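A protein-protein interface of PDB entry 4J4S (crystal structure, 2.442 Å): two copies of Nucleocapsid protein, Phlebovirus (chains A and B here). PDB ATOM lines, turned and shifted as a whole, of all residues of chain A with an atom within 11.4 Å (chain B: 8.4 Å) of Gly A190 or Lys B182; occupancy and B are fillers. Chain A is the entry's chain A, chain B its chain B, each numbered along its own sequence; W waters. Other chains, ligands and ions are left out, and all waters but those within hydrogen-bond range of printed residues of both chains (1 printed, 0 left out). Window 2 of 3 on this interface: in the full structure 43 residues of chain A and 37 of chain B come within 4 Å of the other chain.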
ATOM      1  N   ASP A 178      -7.434   4.371 -32.789  1.00  0.00           N
ATOM      2  CA  ASP A 178      -6.655   3.597 -31.839  1.00  0.00           C
ATOM      3  C   ASP A 178      -7.508   2.547 -31.144  1.00  0.00           C
ATOM      4  O   ASP A 178      -7.110   1.383 -31.005  1.00  0.00           O
ATOM      5  CB  ASP A 178      -6.047   4.538 -30.787  1.00  0.00           C
ATOM      6  CG  ASP A 178      -5.242   3.796 -29.740  1.00  0.00           C
ATOM      7  OD1 ASP A 178      -4.025   3.602 -29.953  1.00  0.00           O
ATOM      8  OD2 ASP A 178      -5.820   3.419 -28.698  1.00  0.00           O
ATOM      9  N   ALA A 179      -8.687   2.973 -30.694  1.00  0.00           N
ATOM     10  CA  ALA A 179      -9.586   2.105 -29.949  1.00  0.00           C
ATOM     11  C   ALA A 179     -10.198   1.065 -30.897  1.00  0.00           C
ATOM     12  O   ALA A 179     -10.259  -0.123 -30.575  1.00  0.00           O
ATOM     13  CB  ALA A 179     -10.658   2.919 -29.282  1.00  0.00           C
ATOM     14  N   THR A 181      -8.882  -0.037 -33.837  1.00  0.00           N
ATOM     15  CA  THR A 181      -7.795  -0.955 -34.204  1.00  0.00           C
ATOM     16  C   THR A 181      -7.614  -2.062 -33.179  1.00  0.00           C
ATOM     17  O   THR A 181      -7.274  -3.189 -33.522  1.00  0.00           O
ATOM     18  CB  THR A 181      -6.442  -0.216 -34.281  1.00  0.00           C
ATOM     19  OG1 THR A 181      -6.556   0.923 -35.133  1.00  0.00           O
ATOM     20  CG2 THR A 181      -5.344  -1.115 -34.803  1.00  0.00           C
ATOM     21  N   LYS A 182      -7.832  -1.748 -31.909  1.00  0.00           N
ATOM     22  CA  LYS A 182      -7.612  -2.730 -30.850  1.00  0.00           C
ATOM     23  C   LYS A 182      -8.761  -3.721 -30.709  1.00  0.00           C
ATOM     24  O   LYS A 182      -8.629  -4.754 -30.057  1.00  0.00           O
ATOM     25  CB  LYS A 182      -7.365  -2.013 -29.542  1.00  0.00           C
ATOM     26  CG  LYS A 182      -6.043  -1.257 -29.541  1.00  0.00           C
ATOM     27  CD  LYS A 182      -5.902  -0.463 -28.283  1.00  0.00           C
ATOM     28  CE  LYS A 182      -4.483   0.018 -28.081  1.00  0.00           C
ATOM     29  NZ  LYS A 182      -4.470   0.822 -26.836  1.00  0.00           N
ATOM     30  N   THR A 183      -9.884  -3.384 -31.337  1.00  0.00           N
ATOM     31  CA  THR A 183     -11.085  -4.205 -31.323  1.00  0.00           C
ATOM     32  C   THR A 183     -11.047  -5.192 -32.485  1.00  0.00           C
ATOM     33  O   THR A 183     -11.472  -6.334 -32.352  1.00  0.00           O
ATOM     34  CB  THR A 183     -12.347  -3.327 -31.430  1.00  0.00           C
ATOM     35  OG1 THR A 183     -12.261  -2.261 -30.476  1.00  0.00           O
ATOM     36  CG2 THR A 183     -13.594  -4.138 -31.135  1.00  0.00           C
ATOM     37  N   ILE A 184     -10.504  -4.724 -33.609  1.00  0.00           N
ATOM     38  CA  ILE A 184     -10.387  -5.458 -34.872  1.00  0.00           C
ATOM     39  C   ILE A 184      -9.184  -6.399 -34.890  1.00  0.00           C
ATOM     40  O   ILE A 184      -9.226  -7.487 -35.460  1.00  0.00           O
ATOM     41  CB  ILE A 184     -10.174  -4.448 -36.014  1.00  0.00           C
ATOM     42  CG1 ILE A 184     -11.347  -3.476 -36.068  1.00  0.00           C
ATOM     43  CG2 ILE A 184      -9.969  -5.154 -37.356  1.00  0.00           C
ATOM     44  CD1 ILE A 184     -12.674  -4.175 -36.224  1.00  0.00           C
ATOM     45  N   ASN A 185      -8.096  -5.935 -34.290  1.00  0.00           N
ATOM     46  CA  ASN A 185      -6.846  -6.661 -34.243  1.00  0.00           C
ATOM     47  C   ASN A 185      -6.425  -6.745 -32.783  1.00  0.00           C
ATOM     48  O   ASN A 185      -5.597  -5.953 -32.309  1.00  0.00           O
ATOM     49  CB  ASN A 185      -5.793  -5.903 -35.045  1.00  0.00           C
ATOM     50  CG  ASN A 185      -4.474  -6.620 -35.087  1.00  0.00           C
ATOM     51  OD1 ASN A 185      -4.342  -7.724 -34.563  1.00  0.00           O
ATOM     52  ND2 ASN A 185      -3.488  -6.007 -35.728  1.00  0.00           N
ATOM     53  N   VAL A 186      -7.010  -7.693 -32.065  1.00  0.00           N
ATOM     54  CA  VAL A 186      -6.719  -7.882 -30.649  1.00  0.00           C
ATOM     55  C   VAL A 186      -5.229  -7.783 -30.295  1.00  0.00           C
ATOM     56  O   VAL A 186      -4.868  -7.312 -29.213  1.00  0.00           O
ATOM     57  CB  VAL A 186      -7.270  -9.213 -30.151  1.00  0.00           C
ATOM     58  CG1 VAL A 186      -7.000  -9.345 -28.671  1.00  0.00           C
ATOM     59  CG2 VAL A 186      -8.765  -9.295 -30.433  1.00  0.00           C
ATOM     60  N   LYS A 187      -4.375  -8.201 -31.220  1.00  0.00           N
ATOM     61  CA  LYS A 187      -2.929  -8.138 -31.019  1.00  0.00           C
ATOM     62  C   LYS A 187      -2.440  -6.733 -30.680  1.00  0.00           C
ATOM     63  O   LYS A 187      -1.458  -6.563 -29.955  1.00  0.00           O
ATOM     64  CB  LYS A 187      -2.198  -8.672 -32.247  1.00  0.00           C
ATOM     65  CG  LYS A 187      -2.390 -10.169 -32.459  1.00  0.00           C
ATOM     66  CD  LYS A 187      -1.234 -10.764 -33.256  1.00  0.00           C
ATOM     67  CE  LYS A 187      -1.576 -10.874 -34.719  1.00  0.00           C
ATOM     68  NZ  LYS A 187      -0.387 -11.224 -35.555  1.00  0.00           N
ATOM     69  N   MET A 188      -3.133  -5.725 -31.195  1.00  0.00           N
ATOM     70  CA  MET A 188      -2.760  -4.336 -30.921  1.00  0.00           C
ATOM     71  C   MET A 188      -3.023  -3.910 -29.470  1.00  0.00           C
ATOM     72  O   MET A 188      -2.727  -2.786 -29.089  1.00  0.00           O
ATOM     73  CB  MET A 188      -3.515  -3.409 -31.869  1.00  0.00           C
ATOM     74  CG  MET A 188      -3.100  -3.562 -33.312  1.00  0.00           C
ATOM     75  SD  MET A 188      -1.439  -2.887 -33.513  1.00  0.00           S
ATOM     76  CE  MET A 188      -1.234  -3.164 -35.281  1.00  0.00           C
ATOM     77  N   ARG A 189      -3.598  -4.806 -28.674  1.00  0.00           N
ATOM     78  CA  ARG A 189      -3.877  -4.518 -27.264  1.00  0.00           C
ATOM     79  C   ARG A 189      -2.563  -4.605 -26.505  1.00  0.00           C
ATOM     80  O   ARG A 189      -2.443  -4.116 -25.387  1.00  0.00           O
ATOM     81  CB  ARG A 189      -4.874  -5.533 -26.702  1.00  0.00           C
ATOM     82  CG  ARG A 189      -5.892  -4.973 -25.755  1.00  0.00           C
ATOM     83  CD  ARG A 189      -7.052  -4.295 -26.472  1.00  0.00           C
ATOM     84  NE  ARG A 189      -8.216  -5.166 -26.590  1.00  0.00           N
ATOM     85  CZ  ARG A 189      -9.465  -4.738 -26.791  1.00  0.00           C
ATOM     86  NH1 ARG A 189      -9.710  -3.431 -26.887  1.00  0.00           N
ATOM     87  NH2 ARG A 189     -10.470  -5.616 -26.890  1.00  0.00           N
ATOM     88  N   GLY A 190      -1.575  -5.235 -27.140  1.00  0.00           N
ATOM     89  CA  GLY A 190      -0.249  -5.370 -26.565  1.00  0.00           C
ATOM     90  C   GLY A 190       0.778  -4.590 -27.359  1.00  0.00           C
ATOM     91  O   GLY A 190       1.979  -4.874 -27.313  1.00  0.00           O
ATOM     92  N   ALA A 191       0.307  -3.596 -28.099  1.00  0.00           N
ATOM     93  CA  ALA A 191       1.210  -2.755 -28.862  1.00  0.00           C
ATOM     94  C   ALA A 191       1.331  -1.362 -28.262  1.00  0.00           C
ATOM     95  O   ALA A 191       0.423  -0.880 -27.579  1.00  0.00           O
ATOM     96  CB  ALA A 191       0.768  -2.664 -30.310  1.00  0.00           C
ATOM     97  N   SER A 192       2.464  -0.731 -28.537  1.00  0.00           N
ATOM     98  CA  SER A 192       2.716   0.647 -28.137  1.00  0.00           C
ATOM     99  C   SER A 192       1.822   1.552 -28.964  1.00  0.00           C
ATOM    100  O   SER A 192       1.408   1.172 -30.076  1.00  0.00           O
ATOM    101  CB  SER A 192       4.167   1.017 -28.437  1.00  0.00           C
ATOM    102  OG  SER A 192       4.403   0.946 -29.837  1.00  0.00           O
ATOM    103  N   LYS A 193       1.558   2.752 -28.452  1.00  0.00           N
ATOM    104  CA  LYS A 193       0.736   3.714 -29.175  1.00  0.00           C
ATOM    105  C   LYS A 193       1.250   3.929 -30.587  1.00  0.00           C
ATOM    106  O   LYS A 193       0.482   3.861 -31.556  1.00  0.00           O
ATOM    107  CB  LYS A 193       0.666   5.044 -28.440  1.00  0.00           C
ATOM    108  CG  LYS A 193      -0.420   5.949 -28.983  1.00  0.00           C
ATOM    109  CD  LYS A 193      -0.512   7.214 -28.163  1.00  0.00           C
ATOM    110  CE  LYS A 193       0.616   8.155 -28.538  1.00  0.00           C
ATOM    111  NZ  LYS A 193       0.323   9.527 -28.034  1.00  0.00           N
ATOM    112  N   THR A 194       2.555   4.162 -30.695  1.00  0.00           N
ATOM    113  CA  THR A 194       3.194   4.409 -31.984  1.00  0.00           C
ATOM    114  C   THR A 194       2.994   3.244 -32.965  1.00  0.00           C
ATOM    115  O   THR A 194       2.603   3.465 -34.116  1.00  0.00           O
ATOM    116  CB  THR A 194       4.685   4.777 -31.818  1.00  0.00           C
ATOM    117  OG1 THR A 194       5.359   3.743 -31.086  1.00  0.00           O
ATOM    118  CG2 THR A 194       4.818   6.102 -31.048  1.00  0.00           C
ATOM    119  N   GLU A 195       3.225   2.014 -32.509  1.00  0.00           N
ATOM    120  CA  GLU A 195       2.964   0.821 -33.338  1.00  0.00           C
ATOM    121  C   GLU A 195       1.516   0.713 -33.830  1.00  0.00           C
ATOM    122  O   GLU A 195       1.257   0.364 -34.988  1.00  0.00           O
ATOM    123  CB  GLU A 195       3.309  -0.457 -32.577  1.00  0.00           C
ATOM    124  CG  GLU A 195       4.781  -0.810 -32.530  1.00  0.00           C
ATOM    125  CD  GLU A 195       5.100  -1.610 -31.280  1.00  0.00           C
ATOM    126  OE1 GLU A 195       4.155  -2.197 -30.683  1.00  0.00           O
ATOM    127  OE2 GLU A 195       6.278  -1.618 -30.867  1.00  0.00           O
ATOM    128  N   VAL A 196       0.575   0.999 -32.945  1.00  0.00           N
ATOM    129  CA  VAL A 196      -0.827   1.055 -33.315  1.00  0.00           C
ATOM    130  C   VAL A 196      -1.035   2.186 -34.316  1.00  0.00           C
ATOM    131  O   VAL A 196      -1.677   2.005 -35.350  1.00  0.00           O
ATOM    132  CB  VAL A 196      -1.721   1.272 -32.086  1.00  0.00           C
ATOM    133  CG1 VAL A 196      -3.176   1.472 -32.502  1.00  0.00           C
ATOM    134  CG2 VAL A 196      -1.567   0.099 -31.102  1.00  0.00           C
ATOM    135  N   TYR A 197      -0.469   3.351 -34.018  1.00  0.00           N
ATOM    136  CA  TYR A 197      -0.586   4.492 -34.910  1.00  0.00           C
ATOM    137  C   TYR A 197      -0.042   4.159 -36.311  1.00  0.00           C
ATOM    138  O   TYR A 197      -0.651   4.532 -37.312  1.00  0.00           O
ATOM    139  CB  TYR A 197       0.117   5.738 -34.319  1.00  0.00           C
ATOM    140  CG  TYR A 197       0.070   6.902 -35.277  1.00  0.00           C
ATOM    141  CD1 TYR A 197      -1.050   7.712 -35.356  1.00  0.00           C
ATOM    142  CD2 TYR A 197       1.120   7.157 -36.141  1.00  0.00           C
ATOM    143  CE1 TYR A 197      -1.116   8.760 -36.255  1.00  0.00           C
ATOM    144  CE2 TYR A 197       1.065   8.200 -37.043  1.00  0.00           C
ATOM    145  CZ  TYR A 197      -0.059   8.998 -37.097  1.00  0.00           C
ATOM    146  OH  TYR A 197      -0.119  10.039 -38.000  1.00  0.00           O
ATOM    147  N   SER A 199      -0.060   1.366 -37.889  1.00  0.00           N
ATOM    148  CA  SER A 199      -0.955   0.457 -38.585  1.00  0.00           C
ATOM    149  C   SER A 199      -2.156   1.152 -39.222  1.00  0.00           C
ATOM    150  O   SER A 199      -2.810   0.576 -40.079  1.00  0.00           O
ATOM    151  CB  SER A 199      -1.432  -0.664 -37.663  1.00  0.00           C
ATOM    152  OG  SER A 199      -2.237  -0.183 -36.598  1.00  0.00           O
ATOM    153  N   VAL B 131      -0.450 -15.860 -16.713  1.00  0.00           N
ATOM    154  CA  VAL B 131      -0.086 -14.479 -16.514  1.00  0.00           C
ATOM    155  C   VAL B 131      -0.709 -13.943 -15.250  1.00  0.00           C
ATOM    156  O   VAL B 131      -1.773 -13.370 -15.274  1.00  0.00           O
ATOM    157  CB  VAL B 131      -0.627 -13.632 -17.641  1.00  0.00           C
ATOM    158  CG1 VAL B 131      -0.761 -12.208 -17.221  1.00  0.00           C
ATOM    159  CG2 VAL B 131       0.249 -13.748 -18.836  1.00  0.00           C
ATOM    160  N   LYS B 139       4.153  -4.685 -11.579  1.00  0.00           N
ATOM    161  CA  LYS B 139       3.584  -3.458 -12.119  1.00  0.00           C
ATOM    162  C   LYS B 139       2.807  -2.658 -11.085  1.00  0.00           C
ATOM    163  O   LYS B 139       2.763  -1.432 -11.157  1.00  0.00           O
ATOM    164  CB  LYS B 139       2.662  -3.767 -13.281  1.00  0.00           C
ATOM    165  CG  LYS B 139       3.303  -4.509 -14.397  1.00  0.00           C
ATOM    166  CD  LYS B 139       2.245  -4.885 -15.407  1.00  0.00           C
ATOM    167  CE  LYS B 139       2.818  -4.867 -16.794  1.00  0.00           C
ATOM    168  NZ  LYS B 139       1.832  -5.412 -17.752  1.00  0.00           N
ATOM    169  N   SER B 174      -7.683  -3.399 -18.190  1.00  0.00           N
ATOM    170  CA  SER B 174      -6.866  -3.283 -19.389  1.00  0.00           C
ATOM    171  C   SER B 174      -5.383  -3.522 -19.058  1.00  0.00           C
ATOM    172  O   SER B 174      -4.637  -4.044 -19.879  1.00  0.00           O
ATOM    173  CB  SER B 174      -7.079  -1.935 -20.086  1.00  0.00           C
ATOM    174  OG  SER B 174      -8.409  -1.804 -20.567  1.00  0.00           O
ATOM    175  N   LEU B 175      -4.983  -3.177 -17.834  1.00  0.00           N
ATOM    176  CA  LEU B 175      -3.617  -3.409 -17.380  1.00  0.00           C
ATOM    177  C   LEU B 175      -3.252  -4.894 -17.449  1.00  0.00           C
ATOM    178  O   LEU B 175      -2.119  -5.234 -17.752  1.00  0.00           O
ATOM    179  CB  LEU B 175      -3.405  -2.851 -15.966  1.00  0.00           C
ATOM    180  CG  LEU B 175      -1.980  -2.645 -15.439  1.00  0.00           C
ATOM    181  CD1 LEU B 175      -1.246  -1.562 -16.225  1.00  0.00           C
ATOM    182  CD2 LEU B 175      -1.999  -2.292 -13.947  1.00  0.00           C
ATOM    183  N   TRP B 176      -4.205  -5.783 -17.191  1.00  0.00           N
ATOM    184  CA  TRP B 176      -3.935  -7.217 -17.306  1.00  0.00           C
ATOM    185  C   TRP B 176      -4.047  -7.716 -18.731  1.00  0.00           C
ATOM    186  O   TRP B 176      -3.198  -8.476 -19.196  1.00  0.00           O
ATOM    187  CB  TRP B 176      -4.870  -8.048 -16.419  1.00  0.00           C
ATOM    188  CG  TRP B 176      -4.654  -9.512 -16.612  1.00  0.00           C
ATOM    189  CD1 TRP B 176      -3.729 -10.298 -15.985  1.00  0.00           C
ATOM    190  CD2 TRP B 176      -5.361 -10.366 -17.514  1.00  0.00           C
ATOM    191  NE1 TRP B 176      -3.813 -11.591 -16.450  1.00  0.00           N
ATOM    192  CE2 TRP B 176      -4.817 -11.658 -17.380  1.00  0.00           C
ATOM    193  CE3 TRP B 176      -6.410 -10.164 -18.411  1.00  0.00           C
ATOM    194  CZ2 TRP B 176      -5.281 -12.735 -18.109  1.00  0.00           C
ATOM    195  CZ3 TRP B 176      -6.857 -11.226 -19.145  1.00  0.00           C
ATOM    196  CH2 TRP B 176      -6.291 -12.499 -18.996  1.00  0.00           C
ATOM    197  N   GLN B 177      -5.114  -7.314 -19.420  1.00  0.00           N
ATOM    198  CA  GLN B 177      -5.320  -7.667 -20.827  1.00  0.00           C
ATOM    199  C   GLN B 177      -4.083  -7.376 -21.654  1.00  0.00           C
ATOM    200  O   GLN B 177      -3.675  -8.163 -22.533  1.00  0.00           O
ATOM    201  CB  GLN B 177      -6.460  -6.836 -21.404  1.00  0.00           C
ATOM    202  CG  GLN B 177      -7.769  -7.563 -21.494  1.00  0.00           C
ATOM    203  CD  GLN B 177      -8.923  -6.644 -21.831  1.00  0.00           C
ATOM    204  OE1 GLN B 177      -8.850  -5.430 -21.621  1.00  0.00           O
ATOM    205  NE2 GLN B 177     -10.000  -7.219 -22.347  1.00  0.00           N
ATOM    206  N   ASP B 178      -3.503  -6.219 -21.387  1.00  0.00           N
ATOM    207  CA  ASP B 178      -2.338  -5.775 -22.130  1.00  0.00           C
ATOM    208  C   ASP B 178      -1.104  -6.632 -21.866  1.00  0.00           C
ATOM    209  O   ASP B 178      -0.453  -7.060 -22.801  1.00  0.00           O
ATOM    210  CB  ASP B 178      -2.099  -4.279 -21.902  1.00  0.00           C
ATOM    211  CG  ASP B 178      -3.216  -3.418 -22.507  1.00  0.00           C
ATOM    212  OD1 ASP B 178      -4.321  -3.959 -22.815  1.00  0.00           O
ATOM    213  OD2 ASP B 178      -2.978  -2.203 -22.688  1.00  0.00           O
ATOM    214  N   ALA B 179      -0.820  -6.932 -20.608  1.00  0.00           N
ATOM    215  CA  ALA B 179       0.259  -7.861 -20.299  1.00  0.00           C
ATOM    216  C   ALA B 179      -0.008  -9.246 -20.886  1.00  0.00           C
ATOM    217  O   ALA B 179       0.901  -9.926 -21.356  1.00  0.00           O
ATOM    218  CB  ALA B 179       0.447  -7.963 -18.818  1.00  0.00           C
ATOM    219  N   PHE B 180      -1.268  -9.656 -20.867  1.00  0.00           N
ATOM    220  CA  PHE B 180      -1.637 -10.976 -21.358  1.00  0.00           C
ATOM    221  C   PHE B 180      -1.563 -11.078 -22.880  1.00  0.00           C
ATOM    222  O   PHE B 180      -1.086 -12.074 -23.427  1.00  0.00           O
ATOM    223  CB  PHE B 180      -3.040 -11.339 -20.851  1.00  0.00           C
ATOM    224  CG  PHE B 180      -3.592 -12.585 -21.456  1.00  0.00           C
ATOM    225  CD1 PHE B 180      -3.227 -13.825 -20.961  1.00  0.00           C
ATOM    226  CD2 PHE B 180      -4.482 -12.520 -22.520  1.00  0.00           C
ATOM    227  CE1 PHE B 180      -3.736 -14.973 -21.502  1.00  0.00           C
ATOM    228  CE2 PHE B 180      -4.997 -13.661 -23.068  1.00  0.00           C
ATOM    229  CZ  PHE B 180      -4.621 -14.893 -22.567  1.00  0.00           C
ATOM    230  N   THR B 181      -2.043 -10.053 -23.571  1.00  0.00           N
ATOM    231  CA  THR B 181      -1.961 -10.033 -25.030  1.00  0.00           C
ATOM    232  C   THR B 181      -0.498 -10.048 -25.506  1.00  0.00           C
ATOM    233  O   THR B 181      -0.199 -10.577 -26.580  1.00  0.00           O
ATOM    234  CB  THR B 181      -2.646  -8.783 -25.612  1.00  0.00           C
ATOM    235  OG1 THR B 181      -3.956  -8.631 -25.060  1.00  0.00           O
ATOM    236  CG2 THR B 181      -2.756  -8.864 -27.098  1.00  0.00           C
ATOM    237  N   LYS B 182       0.422  -9.456 -24.740  1.00  0.00           N
ATOM    238  CA  LYS B 182       1.833  -9.479 -25.162  1.00  0.00           C
ATOM    239  C   LYS B 182       2.412 -10.885 -25.132  1.00  0.00           C
ATOM    240  O   LYS B 182       3.281 -11.214 -25.921  1.00  0.00           O
ATOM    241  CB  LYS B 182       2.722  -8.556 -24.320  1.00  0.00           C
ATOM    242  CG  LYS B 182       2.407  -7.096 -24.479  1.00  0.00           C
ATOM    243  CD  LYS B 182       3.546  -6.232 -23.965  1.00  0.00           C
ATOM    244  CE  LYS B 182       3.106  -4.793 -23.915  1.00  0.00           C
ATOM    245  NZ  LYS B 182       1.832  -4.742 -23.122  1.00  0.00           N
ATOM    246  N   THR B 183       1.945 -11.714 -24.211  1.00  0.00           N
ATOM    247  CA  THR B 183       2.550 -13.026 -24.060  1.00  0.00           C
ATOM    248  C   THR B 183       2.041 -13.922 -25.166  1.00  0.00           C
ATOM    249  O   THR B 183       2.748 -14.830 -25.606  1.00  0.00           O
ATOM    250  CB  THR B 183       2.272 -13.645 -22.674  1.00  0.00           C
ATOM    251  OG1 THR B 183       0.879 -13.946 -22.542  1.00  0.00           O
ATOM    252  CG2 THR B 183       2.688 -12.685 -21.586  1.00  0.00           C
ATOM    253  N   ILE B 184       0.821 -13.624 -25.618  1.00  0.00           N
ATOM    254  CA  ILE B 184       0.162 -14.288 -26.760  1.00  0.00           C
ATOM    255  C   ILE B 184       0.661 -13.805 -28.121  1.00  0.00           C
ATOM    256  O   ILE B 184       0.735 -14.589 -29.078  1.00  0.00           O
ATOM    257  CB  ILE B 184      -1.367 -14.072 -26.717  1.00  0.00           C
ATOM    258  CG1 ILE B 184      -1.955 -14.790 -25.520  1.00  0.00           C
ATOM    259  CG2 ILE B 184      -2.032 -14.617 -27.975  1.00  0.00           C
ATOM    260  CD1 ILE B 184      -1.706 -16.270 -25.564  1.00  0.00           C
ATOM    261  N   ASN B 185       1.004 -12.516 -28.207  1.00  0.00           N
ATOM    262  CA  ASN B 185       1.511 -11.914 -29.446  1.00  0.00           C
ATOM    263  C   ASN B 185       2.855 -12.507 -29.838  1.00  0.00           C
ATOM    264  O   ASN B 185       3.386 -12.257 -30.921  1.00  0.00           O
ATOM    265  CB  ASN B 185       1.673 -10.403 -29.286  1.00  0.00           C
ATOM    266  CG  ASN B 185       0.388  -9.646 -29.518  1.00  0.00           C
ATOM    267  OD1 ASN B 185      -0.667 -10.233 -29.741  1.00  0.00           O
ATOM    268  ND2 ASN B 185       0.474  -8.322 -29.471  1.00  0.00           N
ATOM    269  N   VAL B 186       3.393 -13.316 -28.942  1.00  0.00           N
ATOM    270  CA  VAL B 186       4.767 -13.743 -29.039  1.00  0.00           C
ATOM    271  C   VAL B 186       4.855 -15.280 -29.075  1.00  0.00           C
ATOM    272  O   VAL B 186       5.866 -15.844 -29.486  1.00  0.00           O
ATOM    273  CB  VAL B 186       5.560 -13.074 -27.882  1.00  0.00           C
ATOM    274  CG1 VAL B 186       6.078 -14.081 -26.902  1.00  0.00           C
ATOM    275  CG2 VAL B 186       6.643 -12.164 -28.417  1.00  0.00           C
ATOM    276  N   LYS B 187       3.767 -15.937 -28.668  1.00  0.00           N
ATOM    277  CA  LYS B 187       3.615 -17.398 -28.726  1.00  0.00           C
ATOM    278  C   LYS B 187       3.848 -17.933 -30.142  1.00  0.00           C
ATOM    279  O   LYS B 187       3.398 -17.328 -31.115  1.00  0.00           O
ATOM    280  CB  LYS B 187       2.209 -17.783 -28.258  1.00  0.00           C
ATOM    281  CG  LYS B 187       2.154 -18.812 -27.122  1.00  0.00           C
ATOM    282  CD  LYS B 187       0.887 -18.624 -26.302  1.00  0.00           C
ATOM    283  CE  LYS B 187       0.520 -19.849 -25.463  1.00  0.00           C
ATOM    284  NZ  LYS B 187       1.587 -20.250 -24.491  1.00  0.00           N
ATOM    285  N   PHE B 200     -11.603 -11.521 -26.736  1.00  0.00           N
ATOM    286  CA  PHE B 200     -11.862 -10.705 -25.550  1.00  0.00           C
ATOM    287  C   PHE B 200     -13.300 -10.208 -25.614  1.00  0.00           C
ATOM    288  O   PHE B 200     -13.864 -10.070 -26.697  1.00  0.00           O
ATOM    289  CB  PHE B 200     -10.931  -9.489 -25.523  1.00  0.00           C
ATOM    290  CG  PHE B 200      -9.462  -9.820 -25.339  1.00  0.00           C
ATOM    291  CD1 PHE B 200      -8.853 -10.851 -26.053  1.00  0.00           C
ATOM    292  CD2 PHE B 200      -8.678  -9.055 -24.480  1.00  0.00           C
ATOM    293  CE1 PHE B 200      -7.496 -11.133 -25.879  1.00  0.00           C
ATOM    294  CE2 PHE B 200      -7.320  -9.326 -24.306  1.00  0.00           C
ATOM    295  CZ  PHE B 200      -6.727 -10.358 -25.005  1.00  0.00           C
ATOM    296  N   LEU B 248       0.468   5.030 -18.586  1.00  0.00           N
ATOM    297  CA  LEU B 248       1.074   4.249 -19.633  1.00  0.00           C
ATOM    298  C   LEU B 248       1.761   3.050 -19.073  1.00  0.00           C
ATOM    299  O   LEU B 248       1.607   1.955 -19.594  1.00  0.00           O
ATOM    300  CB  LEU B 248       2.066   5.082 -20.421  1.00  0.00           C
ATOM    301  CG  LEU B 248       3.072   4.321 -21.289  1.00  0.00           C
ATOM    302  CD1 LEU B 248       4.387   5.047 -21.604  1.00  0.00           C
ATOM    303  CD2 LEU B 248       3.339   2.937 -20.742  1.00  0.00           C
HETATM  304  O   HOH W   1       3.379  -7.372 -28.204  1.00  0.00           O
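Water W1 bridges O of Gly A190 and ND2 of Asn B185.
The backbone carbonyl oxygen (O) of Lys A187 is in hydrogen-bond range of the side-chain amide nitrogen (ND2) of Asn B185 (2.7 Å). OD1 of Asp B178 lies close to O of Arg A189, at 3.2 Å.
The side-chain amide oxygen (OD1) of Asn A185 sits close to the backbone NH (N) of Lys A187 (3.4 Å). The side-chain amino group (NZ) of Lys B182 is in hydrogen-bond range of the backbone carbonyl oxygen (O) of Asp B178, 3.3 Å away. The backbone carbonyl oxygen of Thr B181 sits close to the side-chain amide oxygen of Asn B185, 3.2 Å away. The backbone carbonyl oxygen of Gln B177 is in hydrogen-bond range of the side-chain hydroxyl of Thr B181 (2.6 Å).
Of the 20 printed residues of chain A, 4 touch a printed residue of chain B. Hydrophobic or aromatic side chains of chain A within 4 Å of the printed part of chain B: Val A186. Hydrophobic or aromatic side chains of chain B within 4 Å of the printed part of chain A: Phe B200. Among the printed residues, 8 pairs touch across the chains.
Ala A179 touches none of the printed residues of chain B. Of the printed residues of chain B, Val A186 touches Thr B181 and Phe B200. Printed residues of chain B within 4 Å of Lys A187: Thr B181 (3.9 Å) and Asn B185 (2.7 Å). Of the printed residues of chain B, Arg A189 touches Asp B178 (3.1 Å) and Thr B181 (3.6 Å). Of chain B, only Thr B181 and Lys B182 come within 4 Å of Gly A190. No residue of chain B comes within 4 Å of Ala A191. Val A196 touches none of the printed residues of chain B. Of chain A, only Arg A189 (3.1 Å) comes within 4 Å of Asp B178. No residue of chain A comes within 4 Å of Ala B179. Of chain A, only Val A186, Lys A187, Arg A189 and Gly A190 come within 4 Å of Thr B181. Of the printed residues of chain A, Lys B182 touches Gly A190 (3.6 Å). Thr B183 touches none of the printed residues of chain A. Ile B184 touches none of the printed residues of chain A. Of chain A, only Lys A187 (2.7 Å) comes within 4 Å of Asn B185. No residue of chain A comes within 4 Å of Val B186. Of the printed residues of chain A, Phe B200 touches Val A186. The nearest residue of chain B that does not touch Gly A190 is Asp B178 (4.1 Å).
O of Val A186 touches CG2 of Thr B181, at 3.4 Å. Phe B200 touches Val A186 (CE1 to CG1, 3.4 Å). Lys A187 touches Thr B181 (O to CG2, 3.9 Å). CB of Arg A189 touches OG1 of Thr B181, at 3.6 Å. Thr B181 touches Gly A190 (CG2 to N, 3.8 Å). Gly A190 touches Lys B182.
Val A186 touches Thr B181, but with the chains exchanged Thr A181 does not touch Val B186 (15.4 Å). Lys A187 touches Thr B181, but with the chains exchanged Thr A181 does not touch Lys B187 (17.5 Å). Lys A187 touches Asn B185, but with the chains exchanged Asn A185 does not touch Lys B187 (12.8 Å). 9 positions are printed for both chains.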
